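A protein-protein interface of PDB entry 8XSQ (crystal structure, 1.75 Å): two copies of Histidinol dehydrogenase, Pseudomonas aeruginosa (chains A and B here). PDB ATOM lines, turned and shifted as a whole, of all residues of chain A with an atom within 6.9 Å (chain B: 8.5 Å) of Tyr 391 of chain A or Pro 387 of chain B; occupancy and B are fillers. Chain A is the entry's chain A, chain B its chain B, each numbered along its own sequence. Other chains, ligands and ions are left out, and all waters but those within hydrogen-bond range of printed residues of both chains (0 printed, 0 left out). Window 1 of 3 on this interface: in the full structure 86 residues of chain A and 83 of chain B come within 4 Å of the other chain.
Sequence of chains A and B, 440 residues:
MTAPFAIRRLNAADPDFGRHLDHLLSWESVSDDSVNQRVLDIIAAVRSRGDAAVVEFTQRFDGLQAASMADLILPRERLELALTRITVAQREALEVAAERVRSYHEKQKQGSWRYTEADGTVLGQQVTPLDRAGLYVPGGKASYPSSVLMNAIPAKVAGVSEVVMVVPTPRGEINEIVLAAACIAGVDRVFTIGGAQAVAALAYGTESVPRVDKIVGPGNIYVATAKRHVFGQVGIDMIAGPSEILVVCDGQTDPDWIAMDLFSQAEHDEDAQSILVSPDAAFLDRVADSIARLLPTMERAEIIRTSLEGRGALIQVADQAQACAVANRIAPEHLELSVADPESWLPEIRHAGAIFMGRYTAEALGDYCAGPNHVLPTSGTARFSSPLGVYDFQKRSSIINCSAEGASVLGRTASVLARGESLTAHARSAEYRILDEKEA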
ATOM      1  N   HIS A 105      -2.785 -32.621  -3.779  1.00  0.00           N
ATOM      2  CA  HIS A 105      -3.412 -32.218  -2.527  1.00  0.00           C
ATOM      3  C   HIS A 105      -2.449 -31.450  -1.627  1.00  0.00           C
ATOM      4  O   HIS A 105      -2.889 -30.590  -0.857  1.00  0.00           O
ATOM      5  CB  HIS A 105      -3.987 -33.443  -1.817  1.00  0.00           C
ATOM      6  CG  HIS A 105      -5.229 -33.976  -2.464  1.00  0.00           C
ATOM      7  ND1 HIS A 105      -6.391 -33.241  -2.556  1.00  0.00           N
ATOM      8  CD2 HIS A 105      -5.490 -35.165  -3.058  1.00  0.00           C
ATOM      9  CE1 HIS A 105      -7.316 -33.955  -3.174  1.00  0.00           C
ATOM     10  NE2 HIS A 105      -6.794 -35.126  -3.490  1.00  0.00           N
ATOM     11  N   GLN A 108      -2.904 -27.919  -2.622  1.00  0.00           N
ATOM     12  CA  GLN A 108      -4.209 -27.348  -2.321  1.00  0.00           C
ATOM     13  C   GLN A 108      -4.470 -27.190  -0.830  1.00  0.00           C
ATOM     14  O   GLN A 108      -5.434 -26.511  -0.458  1.00  0.00           O
ATOM     15  CB  GLN A 108      -5.313 -28.212  -2.936  1.00  0.00           C
ATOM     16  CG  GLN A 108      -5.394 -28.111  -4.450  1.00  0.00           C
ATOM     17  CD  GLN A 108      -6.210 -26.920  -4.911  1.00  0.00           C
ATOM     18  OE1 GLN A 108      -5.754 -25.779  -4.848  1.00  0.00           O
ATOM     19  NE2 GLN A 108      -7.425 -27.180  -5.382  1.00  0.00           N
ATOM     20  N   LYS A 109      -3.645 -27.793   0.024  1.00  0.00           N
ATOM     21  CA  LYS A 109      -3.884 -27.748   1.459  1.00  0.00           C
ATOM     22  C   LYS A 109      -3.800 -26.317   1.977  1.00  0.00           C
ATOM     23  O   LYS A 109      -2.878 -25.572   1.634  1.00  0.00           O
ATOM     24  CB  LYS A 109      -2.869 -28.629   2.188  1.00  0.00           C
ATOM     25  CG  LYS A 109      -2.930 -28.521   3.705  1.00  0.00           C
ATOM     26  CD  LYS A 109      -2.142 -29.639   4.369  1.00  0.00           C
ATOM     27  CE  LYS A 109      -2.239 -29.567   5.887  1.00  0.00           C
ATOM     28  NZ  LYS A 109      -1.428 -30.633   6.540  1.00  0.00           N
ATOM     29  N   GLN A 110      -4.771 -25.939   2.804  1.00  0.00           N
ATOM     30  CA  GLN A 110      -4.782 -24.647   3.479  1.00  0.00           C
ATOM     31  C   GLN A 110      -4.906 -24.886   4.976  1.00  0.00           C
ATOM     32  O   GLN A 110      -5.856 -25.534   5.427  1.00  0.00           O
ATOM     33  CB  GLN A 110      -5.929 -23.765   2.979  1.00  0.00           C
ATOM     34  CG  GLN A 110      -6.083 -22.460   3.754  1.00  0.00           C
ATOM     35  CD  GLN A 110      -4.936 -21.493   3.516  1.00  0.00           C
ATOM     36  OE1 GLN A 110      -4.686 -21.075   2.385  1.00  0.00           O
ATOM     37  NE2 GLN A 110      -4.231 -21.134   4.583  1.00  0.00           N
ATOM     38  N   GLN A 125      -9.076 -18.284  10.425  1.00  0.00           N
ATOM     39  CA  GLN A 125      -9.621 -19.583  10.778  1.00  0.00           C
ATOM     40  C   GLN A 125      -8.546 -20.410  11.456  1.00  0.00           C
ATOM     41  O   GLN A 125      -7.388 -20.411  11.028  1.00  0.00           O
ATOM     42  CB  GLN A 125     -10.140 -20.333   9.544  1.00  0.00           C
ATOM     43  CG  GLN A 125     -11.297 -19.663   8.831  1.00  0.00           C
ATOM     44  CD  GLN A 125     -11.841 -20.517   7.709  1.00  0.00           C
ATOM     45  OE1 GLN A 125     -13.053 -20.635   7.527  1.00  0.00           O
ATOM     46  NE2 GLN A 125     -10.942 -21.094   6.924  1.00  0.00           N
ATOM     47  N   LEU A 130      -9.170 -33.640  11.130  1.00  0.00           N
ATOM     48  CA  LEU A 130     -10.005 -34.550  11.899  1.00  0.00           C
ATOM     49  C   LEU A 130      -9.132 -35.599  12.577  1.00  0.00           C
ATOM     50  O   LEU A 130      -8.059 -35.956  12.085  1.00  0.00           O
ATOM     51  CB  LEU A 130     -11.042 -35.230  11.004  1.00  0.00           C
ATOM     52  CG  LEU A 130     -12.000 -34.322  10.234  1.00  0.00           C
ATOM     53  CD1 LEU A 130     -12.856 -35.136   9.271  1.00  0.00           C
ATOM     54  CD2 LEU A 130     -12.870 -33.535  11.202  1.00  0.00           C
ATOM     55  N   PRO A 154      -5.848 -37.502   0.533  1.00  0.00           N
ATOM     56  CA  PRO A 154      -6.138 -36.165   1.082  1.00  0.00           C
ATOM     57  C   PRO A 154      -6.346 -36.168   2.585  1.00  0.00           C
ATOM     58  O   PRO A 154      -6.026 -35.172   3.246  1.00  0.00           O
ATOM     59  CB  PRO A 154      -7.412 -35.732   0.339  1.00  0.00           C
ATOM     60  CG  PRO A 154      -7.959 -36.963  -0.278  1.00  0.00           C
ATOM     61  CD  PRO A 154      -6.796 -37.860  -0.538  1.00  0.00           C
ATOM     62  N   ALA A 158      -4.068 -33.889   4.888  1.00  0.00           N
ATOM     63  CA  ALA A 158      -4.667 -32.973   5.853  1.00  0.00           C
ATOM     64  C   ALA A 158      -4.079 -33.157   7.246  1.00  0.00           C
ATOM     65  O   ALA A 158      -4.091 -32.219   8.052  1.00  0.00           O
ATOM     66  CB  ALA A 158      -6.182 -33.169   5.892  1.00  0.00           C
ATOM     67  N   LYS A 214     -15.593 -38.694  10.358  1.00  0.00           N
ATOM     68  CA  LYS A 214     -16.190 -38.577   9.039  1.00  0.00           C
ATOM     69  C   LYS A 214     -16.064 -39.914   8.327  1.00  0.00           C
ATOM     70  O   LYS A 214     -15.048 -40.601   8.461  1.00  0.00           O
ATOM     71  CB  LYS A 214     -15.519 -37.468   8.224  1.00  0.00           C
ATOM     72  CG  LYS A 214     -16.141 -37.227   6.863  1.00  0.00           C
ATOM     73  CD  LYS A 214     -15.544 -35.988   6.229  1.00  0.00           C
ATOM     74  CE  LYS A 214     -16.201 -35.663   4.902  1.00  0.00           C
ATOM     75  NZ  LYS A 214     -16.093 -34.211   4.598  1.00  0.00           N
ATOM     76  N   GLY A 389     -11.735 -33.049  -1.159  1.00  0.00           N
ATOM     77  CA  GLY A 389     -10.296 -32.896  -1.040  1.00  0.00           C
ATOM     78  C   GLY A 389      -9.831 -32.728   0.393  1.00  0.00           C
ATOM     79  O   GLY A 389     -10.517 -33.152   1.324  1.00  0.00           O
ATOM     80  N   VAL A 390      -8.663 -32.100   0.559  1.00  0.00           N
ATOM     81  CA  VAL A 390      -8.080 -31.904   1.886  1.00  0.00           C
ATOM     82  C   VAL A 390      -9.052 -31.166   2.797  1.00  0.00           C
ATOM     83  O   VAL A 390      -9.181 -31.491   3.985  1.00  0.00           O
ATOM     84  CB  VAL A 390      -6.738 -31.156   1.765  1.00  0.00           C
ATOM     85  CG1 VAL A 390      -6.272 -30.649   3.126  1.00  0.00           C
ATOM     86  CG2 VAL A 390      -5.685 -32.048   1.120  1.00  0.00           C
ATOM     87  N   TYR A 391      -9.753 -30.168   2.253  1.00  0.00           N
ATOM     88  CA  TYR A 391     -10.699 -29.387   3.048  1.00  0.00           C
ATOM     89  C   TYR A 391     -11.709 -30.283   3.755  1.00  0.00           C
ATOM     90  O   TYR A 391     -12.103 -30.010   4.895  1.00  0.00           O
ATOM     91  CB  TYR A 391     -11.424 -28.380   2.150  1.00  0.00           C
ATOM     92  CG  TYR A 391     -12.387 -27.466   2.886  1.00  0.00           C
ATOM     93  CD1 TYR A 391     -13.685 -27.876   3.179  1.00  0.00           C
ATOM     94  CD2 TYR A 391     -12.007 -26.182   3.258  1.00  0.00           C
ATOM     95  CE1 TYR A 391     -14.563 -27.046   3.852  1.00  0.00           C
ATOM     96  CE2 TYR A 391     -12.881 -25.342   3.925  1.00  0.00           C
ATOM     97  CZ  TYR A 391     -14.157 -25.780   4.217  1.00  0.00           C
ATOM     98  OH  TYR A 391     -15.036 -24.952   4.877  1.00  0.00           O
ATOM     99  N   ASP A 392     -12.143 -31.356   3.090  1.00  0.00           N
ATOM    100  CA  ASP A 392     -13.150 -32.250   3.647  1.00  0.00           C
ATOM    101  C   ASP A 392     -12.657 -33.015   4.871  1.00  0.00           C
ATOM    102  O   ASP A 392     -13.474 -33.637   5.558  1.00  0.00           O
ATOM    103  CB  ASP A 392     -13.620 -33.242   2.578  1.00  0.00           C
ATOM    104  CG  ASP A 392     -14.475 -32.587   1.501  1.00  0.00           C
ATOM    105  OD1 ASP A 392     -14.953 -31.452   1.707  1.00  0.00           O
ATOM    106  OD2 ASP A 392     -14.652 -33.207   0.431  1.00  0.00           O
ATOM    107  N   PHE A 393     -11.355 -32.987   5.163  1.00  0.00           N
ATOM    108  CA  PHE A 393     -10.799 -33.687   6.313  1.00  0.00           C
ATOM    109  C   PHE A 393     -10.233 -32.729   7.355  1.00  0.00           C
ATOM    110  O   PHE A 393      -9.401 -33.126   8.176  1.00  0.00           O
ATOM    111  CB  PHE A 393      -9.737 -34.684   5.855  1.00  0.00           C
ATOM    112  CG  PHE A 393     -10.274 -35.749   4.938  1.00  0.00           C
ATOM    113  CD1 PHE A 393     -10.952 -36.842   5.454  1.00  0.00           C
ATOM    114  CD2 PHE A 393     -10.122 -35.645   3.566  1.00  0.00           C
ATOM    115  CE1 PHE A 393     -11.454 -37.823   4.622  1.00  0.00           C
ATOM    116  CE2 PHE A 393     -10.625 -36.624   2.724  1.00  0.00           C
ATOM    117  CZ  PHE A 393     -11.293 -37.714   3.254  1.00  0.00           C
ATOM    118  N   GLN A 394     -10.680 -31.480   7.340  1.00  0.00           N
ATOM    119  CA  GLN A 394     -10.268 -30.482   8.310  1.00  0.00           C
ATOM    120  C   GLN A 394     -11.496 -29.928   9.016  1.00  0.00           C
ATOM    121  O   GLN A 394     -12.586 -29.859   8.439  1.00  0.00           O
ATOM    122  CB  GLN A 394      -9.499 -29.338   7.636  1.00  0.00           C
ATOM    123  CG  GLN A 394      -8.257 -29.773   6.871  1.00  0.00           C
ATOM    124  CD  GLN A 394      -7.643 -28.636   6.071  1.00  0.00           C
ATOM    125  OE1 GLN A 394      -8.325 -27.975   5.290  1.00  0.00           O
ATOM    126  NE2 GLN A 394      -6.350 -28.400   6.269  1.00  0.00           N
ATOM    127  N   LYS A 395     -11.319 -29.550  10.277  1.00  0.00           N
ATOM    128  CA  LYS A 395     -12.315 -28.777  11.001  1.00  0.00           C
ATOM    129  C   LYS A 395     -11.833 -27.337  11.095  1.00  0.00           C
ATOM    130  O   LYS A 395     -10.631 -27.081  11.214  1.00  0.00           O
ATOM    131  CB  LYS A 395     -12.569 -29.354  12.398  1.00  0.00           C
ATOM    132  CG  LYS A 395     -11.433 -29.147  13.387  1.00  0.00           C
ATOM    133  CD  LYS A 395     -11.743 -29.793  14.729  1.00  0.00           C
ATOM    134  CE  LYS A 395     -11.645 -31.305  14.642  1.00  0.00           C
ATOM    135  NZ  LYS A 395     -10.238 -31.777  14.780  1.00  0.00           N
ATOM    136  N   ARG A 396     -12.768 -26.396  11.010  1.00  0.00           N
ATOM    137  CA  ARG A 396     -12.427 -24.982  10.983  1.00  0.00           C
ATOM    138  C   ARG A 396     -13.204 -24.229  12.049  1.00  0.00           C
ATOM    139  O   ARG A 396     -14.399 -24.467  12.250  1.00  0.00           O
ATOM    140  CB  ARG A 396     -12.707 -24.365   9.611  1.00  0.00           C
ATOM    141  CG  ARG A 396     -11.895 -24.983   8.495  1.00  0.00           C
ATOM    142  CD  ARG A 396     -12.119 -24.264   7.175  1.00  0.00           C
ATOM    143  NE  ARG A 396     -10.872 -24.026   6.457  1.00  0.00           N
ATOM    144  CZ  ARG A 396     -10.092 -24.977   5.956  1.00  0.00           C
ATOM    145  NH1 ARG A 396     -10.407 -26.258   6.059  1.00  0.00           N
ATOM    146  NH2 ARG A 396      -8.970 -24.631   5.330  1.00  0.00           N
ATOM    147  N   TYR B 104     -17.630  -9.406  -1.188  1.00  0.00           N
ATOM    148  CA  TYR B 104     -16.846 -10.572  -0.795  1.00  0.00           C
ATOM    149  C   TYR B 104     -17.145 -11.764  -1.698  1.00  0.00           C
ATOM    150  O   TYR B 104     -16.228 -12.406  -2.226  1.00  0.00           O
ATOM    151  CB  TYR B 104     -17.139 -10.898   0.672  1.00  0.00           C
ATOM    152  CG  TYR B 104     -16.633 -12.229   1.188  1.00  0.00           C
ATOM    153  CD1 TYR B 104     -15.388 -12.329   1.797  1.00  0.00           C
ATOM    154  CD2 TYR B 104     -17.418 -13.376   1.110  1.00  0.00           C
ATOM    155  CE1 TYR B 104     -14.930 -13.536   2.290  1.00  0.00           C
ATOM    156  CE2 TYR B 104     -16.965 -14.588   1.597  1.00  0.00           C
ATOM    157  CZ  TYR B 104     -15.720 -14.661   2.186  1.00  0.00           C
ATOM    158  OH  TYR B 104     -15.259 -15.861   2.677  1.00  0.00           O
ATOM    159  N   GLN B 108     -14.952 -14.184  -4.594  1.00  0.00           N
ATOM    160  CA  GLN B 108     -14.761 -15.616  -4.409  1.00  0.00           C
ATOM    161  C   GLN B 108     -15.352 -16.451  -5.536  1.00  0.00           C
ATOM    162  O   GLN B 108     -15.018 -17.635  -5.648  1.00  0.00           O
ATOM    163  CB  GLN B 108     -15.373 -16.055  -3.080  1.00  0.00           C
ATOM    164  CG  GLN B 108     -14.779 -15.379  -1.861  1.00  0.00           C
ATOM    165  CD  GLN B 108     -14.572 -16.353  -0.724  1.00  0.00           C
ATOM    166  OE1 GLN B 108     -13.502 -16.400  -0.114  1.00  0.00           O
ATOM    167  NE2 GLN B 108     -15.599 -17.145  -0.435  1.00  0.00           N
ATOM    168  N   LYS B 214     -31.591 -26.883  -2.865  1.00  0.00           N
ATOM    169  CA  LYS B 214     -30.860 -26.757  -1.616  1.00  0.00           C
ATOM    170  C   LYS B 214     -31.653 -25.882  -0.656  1.00  0.00           C
ATOM    171  O   LYS B 214     -32.238 -24.876  -1.063  1.00  0.00           O
ATOM    172  CB  LYS B 214     -29.463 -26.172  -1.854  1.00  0.00           C
ATOM    173  CG  LYS B 214     -28.523 -26.301  -0.675  1.00  0.00           C
ATOM    174  CD  LYS B 214     -27.175 -25.694  -0.994  1.00  0.00           C
ATOM    175  CE  LYS B 214     -26.318 -25.577   0.251  1.00  0.00           C
ATOM    176  NZ  LYS B 214     -24.898 -25.876  -0.059  1.00  0.00           N
ATOM    177  N   ASN B 373     -20.435 -19.363  11.884  1.00  0.00           N
ATOM    178  CA  ASN B 373     -19.064 -19.881  11.826  1.00  0.00           C
ATOM    179  C   ASN B 373     -18.418 -19.598  10.470  1.00  0.00           C
ATOM    180  O   ASN B 373     -17.665 -20.412   9.932  1.00  0.00           O
ATOM    181  CB  ASN B 373     -19.010 -21.374  12.160  1.00  0.00           C
ATOM    182  CG  ASN B 373     -17.603 -21.846  12.494  1.00  0.00           C
ATOM    183  OD1 ASN B 373     -16.755 -21.060  12.919  1.00  0.00           O
ATOM    184  ND2 ASN B 373     -17.354 -23.137  12.307  1.00  0.00           N
ATOM    185  N   HIS B 374     -18.720 -18.433   9.910  1.00  0.00           N
ATOM    186  CA  HIS B 374     -18.031 -17.927   8.734  1.00  0.00           C
ATOM    187  C   HIS B 374     -17.249 -16.679   9.116  1.00  0.00           C
ATOM    188  O   HIS B 374     -17.638 -15.938  10.023  1.00  0.00           O
ATOM    189  CB  HIS B 374     -19.008 -17.612   7.594  1.00  0.00           C
ATOM    190  CG  HIS B 374     -19.997 -18.705   7.321  1.00  0.00           C
ATOM    191  ND1 HIS B 374     -21.274 -18.455   6.865  1.00  0.00           N
ATOM    192  CD2 HIS B 374     -19.894 -20.050   7.434  1.00  0.00           C
ATOM    193  CE1 HIS B 374     -21.916 -19.600   6.711  1.00  0.00           C
ATOM    194  NE2 HIS B 374     -21.101 -20.583   7.050  1.00  0.00           N
ATOM    195  N   PHE B 384      -9.027 -16.026   0.843  1.00  0.00           N
ATOM    196  CA  PHE B 384      -8.968 -17.406   1.310  1.00  0.00           C
ATOM    197  C   PHE B 384     -10.243 -18.120   0.880  1.00  0.00           C
ATOM    198  O   PHE B 384     -11.320 -17.871   1.432  1.00  0.00           O
ATOM    199  CB  PHE B 384      -8.775 -17.456   2.823  1.00  0.00           C
ATOM    200  CG  PHE B 384      -7.448 -16.920   3.273  1.00  0.00           C
ATOM    201  CD1 PHE B 384      -7.267 -15.561   3.474  1.00  0.00           C
ATOM    202  CD2 PHE B 384      -6.372 -17.770   3.469  1.00  0.00           C
ATOM    203  CE1 PHE B 384      -6.045 -15.061   3.876  1.00  0.00           C
ATOM    204  CE2 PHE B 384      -5.145 -17.276   3.871  1.00  0.00           C
ATOM    205  CZ  PHE B 384      -4.982 -15.920   4.076  1.00  0.00           C
ATOM    206  N   SER B 385     -10.112 -19.006  -0.106  1.00  0.00           N
ATOM    207  CA  SER B 385     -11.260 -19.685  -0.684  1.00  0.00           C
ATOM    208  C   SER B 385     -11.950 -20.571   0.349  1.00  0.00           C
ATOM    209  O   SER B 385     -11.389 -20.921   1.391  1.00  0.00           O
ATOM    210  CB  SER B 385     -10.832 -20.523  -1.890  1.00  0.00           C
ATOM    211  OG  SER B 385     -11.616 -21.699  -2.000  1.00  0.00           O
ATOM    212  N   SER B 386     -13.197 -20.934   0.040  1.00  0.00           N
ATOM    213  CA  SER B 386     -14.001 -21.769   0.916  1.00  0.00           C
ATOM    214  C   SER B 386     -15.119 -22.374   0.090  1.00  0.00           C
ATOM    215  O   SER B 386     -15.715 -21.661  -0.729  1.00  0.00           O
ATOM    216  CB  SER B 386     -14.581 -20.962   2.082  1.00  0.00           C
ATOM    217  OG  SER B 386     -15.260 -19.809   1.613  1.00  0.00           O
ATOM    218  N   PRO B 387     -15.429 -23.663   0.259  1.00  0.00           N
ATOM    219  CA  PRO B 387     -16.570 -24.243  -0.468  1.00  0.00           C
ATOM    220  C   PRO B 387     -17.918 -23.714  -0.009  1.00  0.00           C
ATOM    221  O   PRO B 387     -18.929 -24.026  -0.648  1.00  0.00           O
ATOM    222  CB  PRO B 387     -16.449 -25.751  -0.207  1.00  0.00           C
ATOM    223  CG  PRO B 387     -15.371 -25.937   0.763  1.00  0.00           C
ATOM    224  CD  PRO B 387     -14.681 -24.651   1.049  1.00  0.00           C
ATOM    225  N   LEU B 388     -17.978 -22.937   1.069  1.00  0.00           N
ATOM    226  CA  LEU B 388     -19.219 -22.272   1.428  1.00  0.00           C
ATOM    227  C   LEU B 388     -19.407 -21.020   0.574  1.00  0.00           C
ATOM    228  O   LEU B 388     -18.576 -20.674  -0.270  1.00  0.00           O
ATOM    229  CB  LEU B 388     -19.243 -21.937   2.918  1.00  0.00           C
ATOM    230  CG  LEU B 388     -18.652 -22.970   3.879  1.00  0.00           C
ATOM    231  CD1 LEU B 388     -18.487 -22.369   5.267  1.00  0.00           C
ATOM    232  CD2 LEU B 388     -19.525 -24.217   3.932  1.00  0.00           C
ATOM    233  N   GLY B 389     -20.520 -20.331   0.791  1.00  0.00           N
ATOM    234  CA  GLY B 389     -20.803 -19.138   0.012  1.00  0.00           C
ATOM    235  C   GLY B 389     -21.251 -19.498  -1.383  1.00  0.00           C
ATOM    236  O   GLY B 389     -22.118 -20.355  -1.567  1.00  0.00           O
ATOM    237  N   VAL B 390     -20.650 -18.840  -2.379  1.00  0.00           N
ATOM    238  CA  VAL B 390     -21.065 -19.023  -3.768  1.00  0.00           C
ATOM    239  C   VAL B 390     -20.896 -20.476  -4.194  1.00  0.00           C
ATOM    240  O   VAL B 390     -21.731 -21.029  -4.922  1.00  0.00           O
ATOM    241  CB  VAL B 390     -20.282 -18.065  -4.686  1.00  0.00           C
ATOM    242  CG1 VAL B 390     -20.466 -18.441  -6.148  1.00  0.00           C
ATOM    243  CG2 VAL B 390     -20.716 -16.628  -4.443  1.00  0.00           C
ATOM    244  N   TYR B 391     -19.815 -21.119  -3.743  1.00  0.00           N
ATOM    245  CA  TYR B 391     -19.559 -22.514  -4.090  1.00  0.00           C
ATOM    246  C   TYR B 391     -20.723 -23.418  -3.678  1.00  0.00           C
ATOM    247  O   TYR B 391     -21.066 -24.361  -4.401  1.00  0.00           O
ATOM    248  CB  TYR B 391     -18.256 -22.966  -3.429  1.00  0.00           C
ATOM    249  CG  TYR B 391     -17.735 -24.323  -3.856  1.00  0.00           C
ATOM    250  CD1 TYR B 391     -18.202 -25.490  -3.261  1.00  0.00           C
ATOM    251  CD2 TYR B 391     -16.734 -24.434  -4.812  1.00  0.00           C
ATOM    252  CE1 TYR B 391     -17.714 -26.728  -3.635  1.00  0.00           C
ATOM    253  CE2 TYR B 391     -16.239 -25.667  -5.189  1.00  0.00           C
ATOM    254  CZ  TYR B 391     -16.734 -26.810  -4.599  1.00  0.00           C
ATOM    255  OH  TYR B 391     -16.246 -28.041  -4.972  1.00  0.00           O
ATOM    256  N   ASP B 392     -21.342 -23.144  -2.522  1.00  0.00           N
ATOM    257  CA  ASP B 392     -22.499 -23.921  -2.069  1.00  0.00           C
ATOM    258  C   ASP B 392     -23.701 -23.831  -2.999  1.00  0.00           C
ATOM    259  O   ASP B 392     -24.547 -24.730  -2.976  1.00  0.00           O
ATOM    260  CB  ASP B 392     -22.944 -23.493  -0.667  1.00  0.00           C
ATOM    261  CG  ASP B 392     -22.030 -23.999   0.424  1.00  0.00           C
ATOM    262  OD1 ASP B 392     -21.242 -24.929   0.154  1.00  0.00           O
ATOM    263  OD2 ASP B 392     -22.109 -23.473   1.553  1.00  0.00           O
ATOM    264  N   PHE B 393     -23.814 -22.774  -3.800  1.00  0.00           N
ATOM    265  CA  PHE B 393     -24.958 -22.603  -4.685  1.00  0.00           C
ATOM    266  C   PHE B 393     -24.612 -22.915  -6.136  1.00  0.00           C
ATOM    267  O   PHE B 393     -25.319 -22.482  -7.051  1.00  0.00           O
ATOM    268  CB  PHE B 393     -25.509 -21.186  -4.549  1.00  0.00           C
ATOM    269  CG  PHE B 393     -26.043 -20.884  -3.178  1.00  0.00           C
ATOM    270  CD1 PHE B 393     -27.268 -21.386  -2.774  1.00  0.00           C
ATOM    271  CD2 PHE B 393     -25.315 -20.107  -2.291  1.00  0.00           C
ATOM    272  CE1 PHE B 393     -27.762 -21.116  -1.512  1.00  0.00           C
ATOM    273  CE2 PHE B 393     -25.806 -19.831  -1.027  1.00  0.00           C
ATOM    274  CZ  PHE B 393     -27.031 -20.336  -0.639  1.00  0.00           C
ATOM    275  N   GLN B 394     -23.530 -23.654  -6.354  1.00  0.00           N
ATOM    276  CA  GLN B 394     -23.099 -24.060  -7.678  1.00  0.00           C
ATOM    277  C   GLN B 394     -22.994 -25.575  -7.740  1.00  0.00           C
ATOM    278  O   GLN B 394     -22.717 -26.243  -6.739  1.00  0.00           O
ATOM    279  CB  GLN B 394     -21.745 -23.441  -8.042  1.00  0.00           C
ATOM    280  CG  GLN B 394     -21.749 -21.929  -8.147  1.00  0.00           C
ATOM    281  CD  GLN B 394     -20.363 -21.373  -8.391  1.00  0.00           C
ATOM    282  OE1 GLN B 394     -19.386 -21.835  -7.801  1.00  0.00           O
ATOM    283  NE2 GLN B 394     -20.265 -20.381  -9.268  1.00  0.00           N
ATOM    284  N   ARG B 396     -20.844 -28.532  -9.824  1.00  0.00           N
ATOM    285  CA  ARG B 396     -19.606 -28.694 -10.573  1.00  0.00           C
ATOM    286  C   ARG B 396     -19.598 -30.048 -11.263  1.00  0.00           C
ATOM    287  O   ARG B 396     -19.933 -31.069 -10.653  1.00  0.00           O
ATOM    288  CB  ARG B 396     -18.388 -28.540  -9.661  1.00  0.00           C
ATOM    289  CG  ARG B 396     -18.227 -27.120  -9.157  1.00  0.00           C
ATOM    290  CD  ARG B 396     -16.967 -26.920  -8.333  1.00  0.00           C
ATOM    291  NE  ARG B 396     -16.370 -25.607  -8.563  1.00  0.00           N
ATOM    292  CZ  ARG B 396     -16.955 -24.445  -8.294  1.00  0.00           C
ATOM    293  NH1 ARG B 396     -18.155 -24.381  -7.738  1.00  0.00           N
ATOM    294  NH2 ARG B 396     -16.315 -23.316  -8.585  1.00  0.00           N
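Positions printed for both chains: 108, 214, 389, 390, 391, 392, 393, 394 and 396.
Gln 110 of chain A touches Phe 384 of chain B (OE1 to CD2, 3.9 Å). Tyr 391 of chain A touches Pro 387 of chain B (CE1 to CG, 3.4 Å).
Hydrophobic or aromatic side chains of chain B that line the printed part of chain A: Phe 384 and Pro 387. Hydrophobic or aromatic side chains of chain A within 4 Å of the printed part of chain B: Tyr 391.
The side-chain amide nitrogen of Asn 373 of chain B sits at hydrogen-bond distance from the backbone carbonyl oxygen of Arg 396 of chain A.
N of Asp 392 of chain B is in hydrogen-bond range of O of Pro 387 of chain B (3.2 Å). The guanidinium group of Arg 396 of chain A is in hydrogen-bond range of the backbone carbonyl oxygen of Gln 110 of chain A (3.2 Å). NE2 of Gln 394 of chain A lies within hydrogen-bond range of O of Gln 110 of chain A. The side-chain amide nitrogen (NE2) of Gln 125 of chain A sits close to the guanidinium group (NE) of Arg 396 of chain A, at 3.0 Å. O of Phe 384 of chain B lies close to OE1 of Gln 108 of chain B (3.1 Å). The side-chain amide oxygen of Gln 394 of chain A lies within hydrogen-bond range of the guanidinium group of Arg 396 of chain A (2.8 Å).
Tyr 391 of chain A touches one residue of chain B. Of chain A, only Tyr 391 comes within 4 Å of Pro 387 of chain B. Of the printed residues of chain B, Arg 396 of chain A touches Asn 373. Printed residues of chain A within 4 Å of Asn 373 of chain B: Arg 396 (3.2 Å). Of the printed residues of chain B, Gln 110 of chain A touches Phe 384 (3.9 Å). Of the printed residues of chain A, Phe 384 of chain B touches Gln 110 (3.9 Å).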
